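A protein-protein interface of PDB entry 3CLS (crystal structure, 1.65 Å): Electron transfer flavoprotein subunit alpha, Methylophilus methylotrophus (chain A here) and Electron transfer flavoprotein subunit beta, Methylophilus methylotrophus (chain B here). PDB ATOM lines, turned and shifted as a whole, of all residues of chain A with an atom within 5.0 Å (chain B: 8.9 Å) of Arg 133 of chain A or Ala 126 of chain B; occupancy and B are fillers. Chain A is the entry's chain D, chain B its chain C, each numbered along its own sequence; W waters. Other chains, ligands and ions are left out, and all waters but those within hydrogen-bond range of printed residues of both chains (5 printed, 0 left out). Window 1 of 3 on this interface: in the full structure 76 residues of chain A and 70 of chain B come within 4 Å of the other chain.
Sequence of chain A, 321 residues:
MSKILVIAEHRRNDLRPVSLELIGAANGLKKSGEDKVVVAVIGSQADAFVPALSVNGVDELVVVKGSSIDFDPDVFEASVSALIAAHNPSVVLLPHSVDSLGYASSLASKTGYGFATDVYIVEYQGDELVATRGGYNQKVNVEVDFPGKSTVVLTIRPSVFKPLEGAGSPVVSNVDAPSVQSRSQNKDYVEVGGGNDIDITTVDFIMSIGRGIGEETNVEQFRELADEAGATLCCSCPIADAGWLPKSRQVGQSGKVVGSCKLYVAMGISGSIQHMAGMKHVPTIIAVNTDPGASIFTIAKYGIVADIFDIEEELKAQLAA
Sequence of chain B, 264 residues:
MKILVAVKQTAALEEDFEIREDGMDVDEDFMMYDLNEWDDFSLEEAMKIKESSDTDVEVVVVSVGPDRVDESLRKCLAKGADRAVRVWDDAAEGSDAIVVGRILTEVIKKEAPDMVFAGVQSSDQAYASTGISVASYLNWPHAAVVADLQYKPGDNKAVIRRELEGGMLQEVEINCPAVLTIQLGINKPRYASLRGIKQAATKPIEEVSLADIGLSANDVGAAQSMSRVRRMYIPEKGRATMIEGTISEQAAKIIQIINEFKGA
O of Gln 125 of chain B sits at hydrogen-bond distance from NH1 of Arg 133 of chain A (2.8 Å). O of Ala 126 of chain B sits at hydrogen-bond distance from NH2 of Arg 133 of chain A, at 3.0 Å. OG1 of Thr 117 of chain A is in hydrogen-bond range of O of Tyr 127 of chain B (2.7 Å). The backbone carbonyl oxygen (O) of Tyr 233 of chain B sits at hydrogen-bond distance from the backbone NH (N) of Asn 141 of chain A (2.8 Å).
The side-chain carboxylate of Asp 124 of chain B is in hydrogen-bond range of the backbone NH of Ala 11 of chain B (3.1 Å). The backbone carbonyl oxygen (O) of Arg 133 of chain A lies within hydrogen-bond range of the side-chain hydroxyl (OH) of Tyr 120 of chain A (3.3 Å). OH of Tyr 120 of chain A lies within hydrogen-bond range of OD1 of Asn 141 of chain A, 2.7 Å away. O of Arg 133 of chain A lies within hydrogen-bond range of N of Val 142 of chain A, at 2.8 Å. The backbone carbonyl oxygen of Val 140 of chain A lies within hydrogen-bond range of the backbone NH of Gly 135 of chain A.
O of Tyr 127 of chain B touches CE1 of His 96 of chain A, 3.98 Å away. Ser 129 of chain B touches Thr 117 of chain A (OG to CG2, 3.4 Å). Asp 124 of chain B touches Gly 135 of chain A (O to C, 3.8 Å). Gln 125 of chain B touches Gly 135 of chain A (OE1 to CA, 3.4 Å). CA of Met 232 of chain B touches O of Asn 141 of chain A, at 3.3 Å. Asn 141 of chain A touches Pro 235 of chain B (OD1 to CG, 3.5 Å). Val 142 of chain A touches Val 229 of chain B (CG1 to CG2, 3.98 Å). CG2 of Val 142 of chain A touches CE of Met 232 of chain B, 3.4 Å away.
Arg 133 of chain A touches just these residues of chain B: Gln 125 (2.8 Å), Ala 126 (3.0 Å) and Tyr 127 (3.6 Å). Of chain A, only Arg 133 comes within 4 Å of Ala 126 of chain B. No residue of chain B comes within 4 Å of Thr 132 of chain A. No residue of chain B comes within 4 Å of Gly 134 of chain A. Of the printed residues of chain A, Tyr 233 of chain B touches Val 140 and Asn 141. Of the printed residues of chain A, Ser 129 of chain B touches Thr 117. Of the printed residues of chain A, Tyr 127 of chain B touches His 96 (3.98 Å), Thr 117 (2.7 Å) and Arg 133 (3.6 Å). Of the printed residues of chain B, Thr 117 of chain A touches Tyr 127 and Ser 129. The nearest residue of chain A that does not touch Ala 126 of chain B is Thr 117 of chain A (4.3 Å). The nearest printed residue of chain A that does not touch Tyr 127 of chain B is Asp 118 of chain A (5.8 Å).
Hydrophobic or aromatic side chains of chain B that line the printed part of chain A: Tyr 127, Val 229, Met 232, Tyr 233 and Pro 235. Of the 14 printed residues of chain A, 7 touch a printed residue of chain B. Hydrophobic or aromatic side chains of chain A that line the printed part of chain B: His 96, Val 140 and Val 142. Among the printed residues, no Asp or Glu carboxylate lies within 4 Å of a Lys or Arg side-chain nitrogen of the other chain.
Water W3 lies within hydrogen-bond range of the side-chain amide nitrogen (NE2) of Gln 121 of chain B, a ring nitrogen (NE2) of His 96 of chain A and the backbone carbonyl oxygen (O) of Ala 126 of chain B. Water W5 lies within hydrogen-bond range of the backbone carbonyl oxygen (O) of Asp 124 of chain B (2.9 Å) and the backbone NH (N) of Gly 135 of chain A (3.4 Å). Water W4 lies within hydrogen-bond range of the backbone carbonyl oxygen of Gly 134 of chain A (2.9 Å), the backbone carbonyl oxygen of Gln 125 of chain B (3.0 Å) and the guanidinium group of Arg 133 of chain A (3.3 Å).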
ATOM      1  N   HIS A  96      -1.755 -10.736  -8.859  1.00  0.00           N
ATOM      2  CA  HIS A  96      -2.627  -9.725  -8.327  1.00  0.00           C
ATOM      3  C   HIS A  96      -1.788  -8.929  -7.292  1.00  0.00           C
ATOM      4  O   HIS A  96      -2.017  -9.002  -6.079  1.00  0.00           O
ATOM      5  CB  HIS A  96      -3.852 -10.262  -7.652  1.00  0.00           C
ATOM      6  CG  HIS A  96      -4.885  -9.208  -7.408  1.00  0.00           C
ATOM      7  ND1 HIS A  96      -5.550  -8.613  -8.453  1.00  0.00           N
ATOM      8  CD2 HIS A  96      -5.401  -8.675  -6.272  1.00  0.00           C
ATOM      9  CE1 HIS A  96      -6.448  -7.781  -7.982  1.00  0.00           C
ATOM     10  NE2 HIS A  96      -6.359  -7.770  -6.664  1.00  0.00           N
ATOM     11  N   ALA A 116     -10.432 -11.180 -15.549  1.00  0.00           N
ATOM     12  CA  ALA A 116     -10.899 -11.300 -14.166  1.00  0.00           C
ATOM     13  C   ALA A 116      -9.685 -11.159 -13.257  1.00  0.00           C
ATOM     14  O   ALA A 116      -8.588 -11.497 -13.623  1.00  0.00           O
ATOM     15  CB  ALA A 116     -11.569 -12.619 -13.920  1.00  0.00           C
ATOM     16  N   THR A 117      -9.919 -10.685 -12.058  1.00  0.00           N
ATOM     17  CA  THR A 117      -8.890 -10.417 -11.084  1.00  0.00           C
ATOM     18  C   THR A 117      -8.970 -11.183  -9.791  1.00  0.00           C
ATOM     19  O   THR A 117     -10.034 -11.644  -9.387  1.00  0.00           O
ATOM     20  CB  THR A 117      -8.830  -8.888 -10.737  1.00  0.00           C
ATOM     21  OG1 THR A 117     -10.020  -8.464 -10.072  1.00  0.00           O
ATOM     22  CG2 THR A 117      -8.586  -8.000 -11.964  1.00  0.00           C
ATOM     23  N   ASP A 118      -7.821 -11.334  -9.162  1.00  0.00           N
ATOM     24  CA  ASP A 118      -7.688 -11.904  -7.842  1.00  0.00           C
ATOM     25  C   ASP A 118      -8.269 -13.302  -7.809  1.00  0.00           C
ATOM     26  O   ASP A 118      -8.989 -13.676  -6.903  1.00  0.00           O
ATOM     27  CB  ASP A 118      -8.254 -10.958  -6.745  1.00  0.00           C
ATOM     28  CG  ASP A 118      -7.852 -11.371  -5.343  1.00  0.00           C
ATOM     29  OD1 ASP A 118      -6.761 -11.986  -5.176  1.00  0.00           O
ATOM     30  OD2 ASP A 118      -8.598 -11.049  -4.383  1.00  0.00           O
ATOM     31  N   VAL A 119      -7.915 -14.074  -8.846  1.00  0.00           N
ATOM     32  CA  VAL A 119      -8.430 -15.417  -9.096  1.00  0.00           C
ATOM     33  C   VAL A 119      -7.698 -16.459  -8.288  1.00  0.00           C
ATOM     34  O   VAL A 119      -6.463 -16.409  -8.197  1.00  0.00           O
ATOM     35  CB  VAL A 119      -8.363 -15.717 -10.646  1.00  0.00           C
ATOM     36  CG1 VAL A 119      -8.571 -17.194 -10.896  1.00  0.00           C
ATOM     37  CG2 VAL A 119      -9.375 -14.846 -11.360  1.00  0.00           C
ATOM     38  N   TYR A 120      -8.447 -17.337  -7.627  1.00  0.00           N
ATOM     39  CA  TYR A 120      -7.825 -18.388  -6.790  1.00  0.00           C
ATOM     40  C   TYR A 120      -8.183 -19.828  -7.127  1.00  0.00           C
ATOM     41  O   TYR A 120      -7.747 -20.753  -6.439  1.00  0.00           O
ATOM     42  CB  TYR A 120      -8.027 -18.070  -5.315  1.00  0.00           C
ATOM     43  CG  TYR A 120      -9.394 -17.752  -4.896  1.00  0.00           C
ATOM     44  CD1 TYR A 120     -10.273 -18.770  -4.565  1.00  0.00           C
ATOM     45  CD2 TYR A 120      -9.823 -16.429  -4.762  1.00  0.00           C
ATOM     46  CE1 TYR A 120     -11.573 -18.489  -4.120  1.00  0.00           C
ATOM     47  CE2 TYR A 120     -11.172 -16.151  -4.323  1.00  0.00           C
ATOM     48  CZ  TYR A 120     -11.986 -17.167  -3.975  1.00  0.00           C
ATOM     49  OH  TYR A 120     -13.264 -16.900  -3.501  1.00  0.00           O
ATOM     50  N   ALA A 131     -12.799 -19.601 -14.233  1.00  0.00           N
ATOM     51  CA  ALA A 131     -12.016 -18.998 -13.172  1.00  0.00           C
ATOM     52  C   ALA A 131     -12.921 -18.702 -12.030  1.00  0.00           C
ATOM     53  O   ALA A 131     -14.079 -18.321 -12.270  1.00  0.00           O
ATOM     54  CB  ALA A 131     -11.396 -17.683 -13.659  1.00  0.00           C
ATOM     55  N   THR A 132     -12.388 -18.797 -10.807  1.00  0.00           N
ATOM     56  CA  THR A 132     -13.170 -18.478  -9.582  1.00  0.00           C
ATOM     57  C   THR A 132     -12.465 -17.379  -8.780  1.00  0.00           C
ATOM     58  O   THR A 132     -11.276 -17.423  -8.531  1.00  0.00           O
ATOM     59  CB  THR A 132     -13.403 -19.689  -8.711  1.00  0.00           C
ATOM     60  OG1 THR A 132     -13.966 -20.727  -9.522  1.00  0.00           O
ATOM     61  CG2 THR A 132     -14.374 -19.375  -7.516  1.00  0.00           C
ATOM     62  N   ARG A 133     -13.254 -16.400  -8.385  1.00  0.00           N
ATOM     63  CA  ARG A 133     -12.791 -15.334  -7.511  1.00  0.00           C
ATOM     64  C   ARG A 133     -13.795 -15.173  -6.382  1.00  0.00           C
ATOM     65  O   ARG A 133     -14.781 -15.901  -6.304  1.00  0.00           O
ATOM     66  CB  ARG A 133     -12.634 -14.045  -8.308  1.00  0.00           C
ATOM     67  CG  ARG A 133     -14.013 -13.416  -8.778  1.00  0.00           C
ATOM     68  CD  ARG A 133     -13.862 -12.252  -9.687  1.00  0.00           C
ATOM     69  NE  ARG A 133     -12.840 -11.271  -9.254  1.00  0.00           N
ATOM     70  CZ  ARG A 133     -12.975 -10.420  -8.250  1.00  0.00           C
ATOM     71  NH1 ARG A 133     -14.138 -10.318  -7.630  1.00  0.00           N
ATOM     72  NH2 ARG A 133     -11.982  -9.574  -7.927  1.00  0.00           N
ATOM     73  N   GLY A 134     -13.550 -14.189  -5.517  1.00  0.00           N
ATOM     74  CA  GLY A 134     -14.474 -13.959  -4.382  1.00  0.00           C
ATOM     75  C   GLY A 134     -15.612 -13.010  -4.690  1.00  0.00           C
ATOM     76  O   GLY A 134     -15.593 -12.269  -5.696  1.00  0.00           O
ATOM     77  N   GLY A 135     -16.637 -13.021  -3.851  1.00  0.00           N
ATOM     78  CA  GLY A 135     -17.718 -12.003  -3.904  1.00  0.00           C
ATOM     79  C   GLY A 135     -18.056 -11.609  -2.472  1.00  0.00           C
ATOM     80  O   GLY A 135     -17.939 -12.431  -1.532  1.00  0.00           O
ATOM     81  N   VAL A 140     -18.793 -15.293  -0.669  1.00  0.00           N
ATOM     82  CA  VAL A 140     -19.084 -16.241  -1.709  1.00  0.00           C
ATOM     83  C   VAL A 140     -17.900 -16.477  -2.660  1.00  0.00           C
ATOM     84  O   VAL A 140     -16.928 -15.637  -2.730  1.00  0.00           O
ATOM     85  CB  VAL A 140     -20.341 -15.858  -2.550  1.00  0.00           C
ATOM     86  CG1 VAL A 140     -21.580 -15.663  -1.685  1.00  0.00           C
ATOM     87  CG2 VAL A 140     -20.120 -14.553  -3.343  1.00  0.00           C
ATOM     88  N   ASN A 141     -18.031 -17.576  -3.437  1.00  0.00           N
ATOM     89  CA  ASN A 141     -17.246 -17.807  -4.636  1.00  0.00           C
ATOM     90  C   ASN A 141     -18.074 -17.351  -5.830  1.00  0.00           C
ATOM     91  O   ASN A 141     -19.247 -17.683  -5.928  1.00  0.00           O
ATOM     92  CB  ASN A 141     -16.859 -19.282  -4.804  1.00  0.00           C
ATOM     93  CG  ASN A 141     -15.610 -19.622  -3.984  1.00  0.00           C
ATOM     94  OD1 ASN A 141     -15.155 -18.783  -3.190  1.00  0.00           O
ATOM     95  ND2 ASN A 141     -15.127 -20.838  -4.107  1.00  0.00           N
ATOM     96  N   VAL A 142     -17.413 -16.659  -6.749  1.00  0.00           N
ATOM     97  CA  VAL A 142     -18.005 -16.273  -8.041  1.00  0.00           C
ATOM     98  C   VAL A 142     -17.218 -16.984  -9.144  1.00  0.00           C
ATOM     99  O   VAL A 142     -16.042 -16.718  -9.337  1.00  0.00           O
ATOM    100  CB  VAL A 142     -17.976 -14.707  -8.261  1.00  0.00           C
ATOM    101  CG1 VAL A 142     -18.791 -14.308  -9.503  1.00  0.00           C
ATOM    102  CG2 VAL A 142     -18.554 -14.019  -6.987  1.00  0.00           C
ATOM    103  N   LYS B   8     -18.437   4.384  -4.997  1.00  0.00           N
ATOM    104  CA  LYS B   8     -19.310   3.213  -5.085  1.00  0.00           C
ATOM    105  C   LYS B   8     -20.007   2.992  -3.738  1.00  0.00           C
ATOM    106  O   LYS B   8     -19.376   3.044  -2.679  1.00  0.00           O
ATOM    107  CB  LYS B   8     -18.505   1.984  -5.424  1.00  0.00           C
ATOM    108  CG  LYS B   8     -19.439   0.775  -5.630  1.00  0.00           C
ATOM    109  CD  LYS B   8     -18.667  -0.493  -5.883  1.00  0.00           C
ATOM    110  CE  LYS B   8     -19.533  -1.700  -6.127  1.00  0.00           C
ATOM    111  NZ  LYS B   8     -18.813  -3.030  -6.323  1.00  0.00           N
ATOM    112  N   THR B  10     -21.267   0.165  -1.757  1.00  0.00           N
ATOM    113  CA  THR B  10     -20.995  -1.289  -1.662  1.00  0.00           C
ATOM    114  C   THR B  10     -22.058  -1.984  -0.834  1.00  0.00           C
ATOM    115  O   THR B  10     -22.772  -1.357  -0.025  1.00  0.00           O
ATOM    116  CB  THR B  10     -19.587  -1.515  -1.045  1.00  0.00           C
ATOM    117  OG1 THR B  10     -19.452  -0.718   0.164  1.00  0.00           O
ATOM    118  CG2 THR B  10     -18.526  -1.139  -2.072  1.00  0.00           C
ATOM    119  N   ALA B  11     -22.169  -3.298  -1.032  1.00  0.00           N
ATOM    120  CA  ALA B  11     -23.122  -4.127  -0.310  1.00  0.00           C
ATOM    121  C   ALA B  11     -22.341  -5.054   0.592  1.00  0.00           C
ATOM    122  O   ALA B  11     -21.337  -5.682   0.156  1.00  0.00           O
ATOM    123  CB  ALA B  11     -23.983  -4.905  -1.284  1.00  0.00           C
ATOM    124  N   ASN B  36     -18.329   2.818  -0.011  1.00  0.00           N
ATOM    125  CA  ASN B  36     -17.083   2.046  -0.005  1.00  0.00           C
ATOM    126  C   ASN B  36     -16.064   2.717   0.891  1.00  0.00           C
ATOM    127  O   ASN B  36     -15.858   3.940   0.789  1.00  0.00           O
ATOM    128  CB  ASN B  36     -16.555   1.931  -1.418  1.00  0.00           C
ATOM    129  CG  ASN B  36     -15.340   1.016  -1.522  1.00  0.00           C
ATOM    130  OD1 ASN B  36     -15.221  -0.012  -0.807  1.00  0.00           O
ATOM    131  ND2 ASN B  36     -14.472   1.382  -2.443  1.00  0.00           N
ATOM    132  N   TRP B  38     -12.873   2.840   0.869  1.00  0.00           N
ATOM    133  CA  TRP B  38     -11.750   3.523   0.160  1.00  0.00           C
ATOM    134  C   TRP B  38     -12.238   4.892  -0.272  1.00  0.00           C
ATOM    135  O   TRP B  38     -11.466   5.889  -0.352  1.00  0.00           O
ATOM    136  CB  TRP B  38     -11.324   2.712  -1.048  1.00  0.00           C
ATOM    137  CG  TRP B  38     -10.310   1.645  -0.679  1.00  0.00           C
ATOM    138  CD1 TRP B  38      -8.975   1.769  -0.685  1.00  0.00           C
ATOM    139  CD2 TRP B  38     -10.590   0.360  -0.116  1.00  0.00           C
ATOM    140  NE1 TRP B  38      -8.367   0.631  -0.213  1.00  0.00           N
ATOM    141  CE2 TRP B  38      -9.334  -0.267   0.132  1.00  0.00           C
ATOM    142  CE3 TRP B  38     -11.761  -0.352   0.140  1.00  0.00           C
ATOM    143  CZ2 TRP B  38      -9.250  -1.508   0.713  1.00  0.00           C
ATOM    144  CZ3 TRP B  38     -11.668  -1.580   0.698  1.00  0.00           C
ATOM    145  CH2 TRP B  38     -10.431  -2.164   0.951  1.00  0.00           C
ATOM    146  N   ALA B  97     -16.345  -3.992 -13.916  1.00  0.00           N
ATOM    147  CA  ALA B  97     -15.458  -2.858 -13.612  1.00  0.00           C
ATOM    148  C   ALA B  97     -15.183  -2.118 -14.911  1.00  0.00           C
ATOM    149  O   ALA B  97     -15.108  -0.938 -14.900  1.00  0.00           O
ATOM    150  CB  ALA B  97     -14.231  -3.298 -12.972  1.00  0.00           C
ATOM    151  N   VAL B 120      -8.738   2.324  -4.352  1.00  0.00           N
ATOM    152  CA  VAL B 120      -7.962   1.136  -4.781  1.00  0.00           C
ATOM    153  C   VAL B 120      -8.868  -0.034  -5.152  1.00  0.00           C
ATOM    154  O   VAL B 120      -8.629  -0.698  -6.154  1.00  0.00           O
ATOM    155  CB  VAL B 120      -6.971   0.674  -3.688  1.00  0.00           C
ATOM    156  CG1 VAL B 120      -6.423  -0.690  -3.975  1.00  0.00           C
ATOM    157  CG2 VAL B 120      -5.851   1.636  -3.646  1.00  0.00           C
ATOM    158  N   GLN B 121      -9.895  -0.281  -4.340  1.00  0.00           N
ATOM    159  CA  GLN B 121     -10.788  -1.408  -4.624  1.00  0.00           C
ATOM    160  C   GLN B 121     -12.101  -1.218  -3.869  1.00  0.00           C
ATOM    161  O   GLN B 121     -12.188  -0.372  -2.970  1.00  0.00           O
ATOM    162  CB  GLN B 121     -10.176  -2.746  -4.232  1.00  0.00           C
ATOM    163  CG  GLN B 121      -9.961  -2.971  -2.729  1.00  0.00           C
ATOM    164  CD  GLN B 121      -9.366  -4.336  -2.405  1.00  0.00           C
ATOM    165  OE1 GLN B 121      -9.790  -4.996  -1.457  1.00  0.00           O
ATOM    166  NE2 GLN B 121      -8.413  -4.753  -3.200  1.00  0.00           N
ATOM    167  N   SER B 122     -13.088  -2.024  -4.235  1.00  0.00           N
ATOM    168  CA  SER B 122     -14.386  -2.048  -3.514  1.00  0.00           C
ATOM    169  C   SER B 122     -14.391  -3.154  -2.455  1.00  0.00           C
ATOM    170  O   SER B 122     -13.848  -4.240  -2.636  1.00  0.00           O
ATOM    171  CB  SER B 122     -15.565  -2.313  -4.485  1.00  0.00           C
ATOM    172  OG  SER B 122     -15.290  -3.423  -5.320  1.00  0.00           O
ATOM    173  N   SER B 123     -15.026  -2.856  -1.342  1.00  0.00           N
ATOM    174  CA  SER B 123     -15.053  -3.819  -0.242  1.00  0.00           C
ATOM    175  C   SER B 123     -15.868  -5.072  -0.567  1.00  0.00           C
ATOM    176  O   SER B 123     -15.602  -6.141   0.052  1.00  0.00           O
ATOM    177  CB  SER B 123     -15.531  -3.169   1.060  1.00  0.00           C
ATOM    178  OG  SER B 123     -16.862  -2.742   0.934  1.00  0.00           O
ATOM    179  N   ASP B 124     -16.850  -4.936  -1.476  1.00  0.00           N
ATOM    180  CA  ASP B 124     -17.647  -6.061  -1.834  1.00  0.00           C
ATOM    181  C   ASP B 124     -16.949  -6.970  -2.814  1.00  0.00           C
ATOM    182  O   ASP B 124     -16.626  -8.126  -2.469  1.00  0.00           O
ATOM    183  CB  ASP B 124     -19.095  -5.674  -2.239  1.00  0.00           C
ATOM    184  CG  ASP B 124     -19.192  -4.507  -3.208  1.00  0.00           C
ATOM    185  OD1 ASP B 124     -18.170  -4.127  -3.813  1.00  0.00           O
ATOM    186  OD2 ASP B 124     -20.348  -4.002  -3.382  1.00  0.00           O
ATOM    187  N   GLN B 125     -16.726  -6.488  -4.036  1.00  0.00           N
ATOM    188  CA  GLN B 125     -16.173  -7.347  -5.104  1.00  0.00           C
ATOM    189  C   GLN B 125     -14.664  -7.315  -5.170  1.00  0.00           C
ATOM    190  O   GLN B 125     -14.045  -8.208  -5.724  1.00  0.00           O
ATOM    191  CB  GLN B 125     -16.732  -6.917  -6.438  1.00  0.00           C
ATOM    192  CG  GLN B 125     -18.306  -6.928  -6.474  1.00  0.00           C
ATOM    193  CD  GLN B 125     -19.159  -7.930  -5.477  1.00  0.00           C
ATOM    194  OE1 GLN B 125     -18.681  -8.938  -4.937  1.00  0.00           O
ATOM    195  NE2 GLN B 125     -20.451  -7.606  -5.298  1.00  0.00           N
ATOM    196  N   ALA B 126     -14.080  -6.223  -4.710  1.00  0.00           N
ATOM    197  CA  ALA B 126     -12.616  -6.119  -4.634  1.00  0.00           C
ATOM    198  C   ALA B 126     -12.012  -6.494  -5.993  1.00  0.00           C
ATOM    199  O   ALA B 126     -11.098  -7.348  -6.067  1.00  0.00           O
ATOM    200  CB  ALA B 126     -12.112  -7.008  -3.545  1.00  0.00           C
ATOM    201  N   TYR B 127     -12.522  -5.868  -7.044  1.00  0.00           N
ATOM    202  CA  TYR B 127     -11.949  -6.048  -8.420  1.00  0.00           C
ATOM    203  C   TYR B 127     -10.552  -5.385  -8.539  1.00  0.00           C
ATOM    204  O   TYR B 127      -9.686  -5.862  -9.283  1.00  0.00           O
ATOM    205  CB  TYR B 127     -12.887  -5.467  -9.471  1.00  0.00           C
ATOM    206  CG  TYR B 127     -14.242  -6.064  -9.590  1.00  0.00           C
ATOM    207  CD1 TYR B 127     -15.352  -5.256  -9.555  1.00  0.00           C
ATOM    208  CD2 TYR B 127     -14.446  -7.448  -9.716  1.00  0.00           C
ATOM    209  CE1 TYR B 127     -16.596  -5.738  -9.717  1.00  0.00           C
ATOM    210  CE2 TYR B 127     -15.711  -7.955  -9.859  1.00  0.00           C
ATOM    211  CZ  TYR B 127     -16.803  -7.090  -9.780  1.00  0.00           C
ATOM    212  OH  TYR B 127     -18.126  -7.509  -9.872  1.00  0.00           O
ATOM    213  N   ALA B 128     -10.386  -4.245  -7.847  1.00  0.00           N
ATOM    214  CA  ALA B 128      -9.201  -3.338  -7.979  1.00  0.00           C
ATOM    215  C   ALA B 128      -8.966  -3.088  -9.468  1.00  0.00           C
ATOM    216  O   ALA B 128      -7.823  -3.230  -9.960  1.00  0.00           O
ATOM    217  CB  ALA B 128      -7.949  -3.921  -7.303  1.00  0.00           C
ATOM    218  N   SER B 129     -10.052  -2.745 -10.182  1.00  0.00           N
ATOM    219  CA  SER B 129      -9.973  -2.527 -11.649  1.00  0.00           C
ATOM    220  C   SER B 129     -10.601  -1.244 -12.162  1.00  0.00           C
ATOM    221  O   SER B 129     -10.255  -0.768 -13.241  1.00  0.00           O
ATOM    222  CB  SER B 129     -10.732  -3.659 -12.320  1.00  0.00           C
ATOM    223  OG  SER B 129     -10.017  -4.875 -12.140  1.00  0.00           O
ATOM    224  N   THR B 130     -11.618  -0.753 -11.469  1.00  0.00           N
ATOM    225  CA  THR B 130     -12.492   0.296 -12.053  1.00  0.00           C
ATOM    226  C   THR B 130     -11.743   1.635 -12.354  1.00  0.00           C
ATOM    227  O   THR B 130     -11.823   2.159 -13.468  1.00  0.00           O
ATOM    228  CB  THR B 130     -13.719   0.532 -11.187  1.00  0.00           C
ATOM    229  OG1 THR B 130     -14.411  -0.727 -10.984  1.00  0.00           O
ATOM    230  CG2 THR B 130     -14.614   1.531 -11.792  1.00  0.00           C
ATOM    231  N   SER B 227     -16.142 -10.749 -18.479  1.00  0.00           N
ATOM    232  CA  SER B 227     -16.327 -12.156 -18.069  1.00  0.00           C
ATOM    233  C   SER B 227     -17.809 -12.333 -17.818  1.00  0.00           C
ATOM    234  O   SER B 227     -18.523 -11.322 -17.645  1.00  0.00           O
ATOM    235  CB  SER B 227     -15.581 -12.464 -16.783  1.00  0.00           C
ATOM    236  OG  SER B 227     -15.989 -11.612 -15.699  1.00  0.00           O
ATOM    237  N   VAL B 229     -20.638 -14.340 -15.422  1.00  0.00           N
ATOM    238  CA  VAL B 229     -20.900 -15.045 -14.181  1.00  0.00           C
ATOM    239  C   VAL B 229     -21.651 -16.325 -14.518  1.00  0.00           C
ATOM    240  O   VAL B 229     -22.742 -16.290 -15.105  1.00  0.00           O
ATOM    241  CB  VAL B 229     -21.683 -14.169 -13.128  1.00  0.00           C
ATOM    242  CG1 VAL B 229     -22.164 -15.069 -11.960  1.00  0.00           C
ATOM    243  CG2 VAL B 229     -20.815 -13.035 -12.687  1.00  0.00           C
ATOM    244  N   ARG B 231     -22.052 -18.843 -11.896  1.00  0.00           N
ATOM    245  CA  ARG B 231     -22.793 -18.993 -10.664  1.00  0.00           C
ATOM    246  C   ARG B 231     -22.055 -18.262  -9.560  1.00  0.00           C
ATOM    247  O   ARG B 231     -20.871 -17.977  -9.666  1.00  0.00           O
ATOM    248  CB  ARG B 231     -22.960 -20.485 -10.278  1.00  0.00           C
ATOM    249  CG  ARG B 231     -21.616 -21.201 -10.062  1.00  0.00           C
ATOM    250  CD  ARG B 231     -21.802 -22.624  -9.536  1.00  0.00           C
ATOM    251  NE  ARG B 231     -20.533 -23.349  -9.578  1.00  0.00           N
ATOM    252  CZ  ARG B 231     -20.117 -24.237  -8.693  1.00  0.00           C
ATOM    253  NH1 ARG B 231     -20.877 -24.564  -7.663  1.00  0.00           N
ATOM    254  NH2 ARG B 231     -18.928 -24.795  -8.859  1.00  0.00           N
ATOM    255  N   MET B 232     -22.790 -18.128  -8.475  1.00  0.00           N
ATOM    256  CA  MET B 232     -22.266 -17.647  -7.247  1.00  0.00           C
ATOM    257  C   MET B 232     -22.732 -18.660  -6.203  1.00  0.00           C
ATOM    258  O   MET B 232     -23.884 -19.132  -6.206  1.00  0.00           O
ATOM    259  CB  MET B 232     -22.830 -16.271  -7.027  1.00  0.00           C
ATOM    260  CG  MET B 232     -22.205 -15.529  -5.914  1.00  0.00           C
ATOM    261  SD  MET B 232     -22.917 -13.881  -5.774  1.00  0.00           S
ATOM    262  CE  MET B 232     -21.784 -12.866  -6.692  1.00  0.00           C
ATOM    263  N   TYR B 233     -21.815 -19.015  -5.313  1.00  0.00           N
ATOM    264  CA  TYR B 233     -22.053 -20.052  -4.350  1.00  0.00           C
ATOM    265  C   TYR B 233     -21.315 -19.816  -3.053  1.00  0.00           C
ATOM    266  O   TYR B 233     -20.322 -19.116  -3.052  1.00  0.00           O
ATOM    267  CB  TYR B 233     -21.782 -21.465  -4.942  1.00  0.00           C
ATOM    268  CG  TYR B 233     -20.350 -21.782  -5.260  1.00  0.00           C
ATOM    269  CD1 TYR B 233     -19.513 -22.418  -4.327  1.00  0.00           C
ATOM    270  CD2 TYR B 233     -19.786 -21.395  -6.486  1.00  0.00           C
ATOM    271  CE1 TYR B 233     -18.172 -22.674  -4.602  1.00  0.00           C
ATOM    272  CE2 TYR B 233     -18.470 -21.656  -6.764  1.00  0.00           C
ATOM    273  CZ  TYR B 233     -17.675 -22.321  -5.842  1.00  0.00           C
ATOM    274  OH  TYR B 233     -16.391 -22.600  -6.164  1.00  0.00           O
ATOM    275  N   PRO B 235     -18.958 -21.350  -0.640  1.00  0.00           N
ATOM    276  CA  PRO B 235     -18.051 -22.515  -0.683  1.00  0.00           C
ATOM    277  C   PRO B 235     -17.956 -23.142   0.721  1.00  0.00           C
ATOM    278  O   PRO B 235     -18.192 -22.467   1.752  1.00  0.00           O
ATOM    279  CB  PRO B 235     -16.723 -21.903  -1.108  1.00  0.00           C
ATOM    280  CG  PRO B 235     -16.761 -20.431  -0.545  1.00  0.00           C
ATOM    281  CD  PRO B 235     -18.235 -20.066  -0.551  1.00  0.00           C
HETATM  282  O   HOH W   1     -10.845  -9.956  -4.790  1.00  0.00           O
HETATM  283  O   HOH W   2     -15.813 -22.518  -8.671  1.00  0.00           O
HETATM  284  O   HOH W   3      -8.409  -6.849  -4.973  1.00  0.00           O
HETATM  285  O   HOH W   4     -13.348 -10.825  -4.504  1.00  0.00           O
HETATM  286  O   HOH W   5     -15.040 -10.497  -2.225  1.00  0.00           O
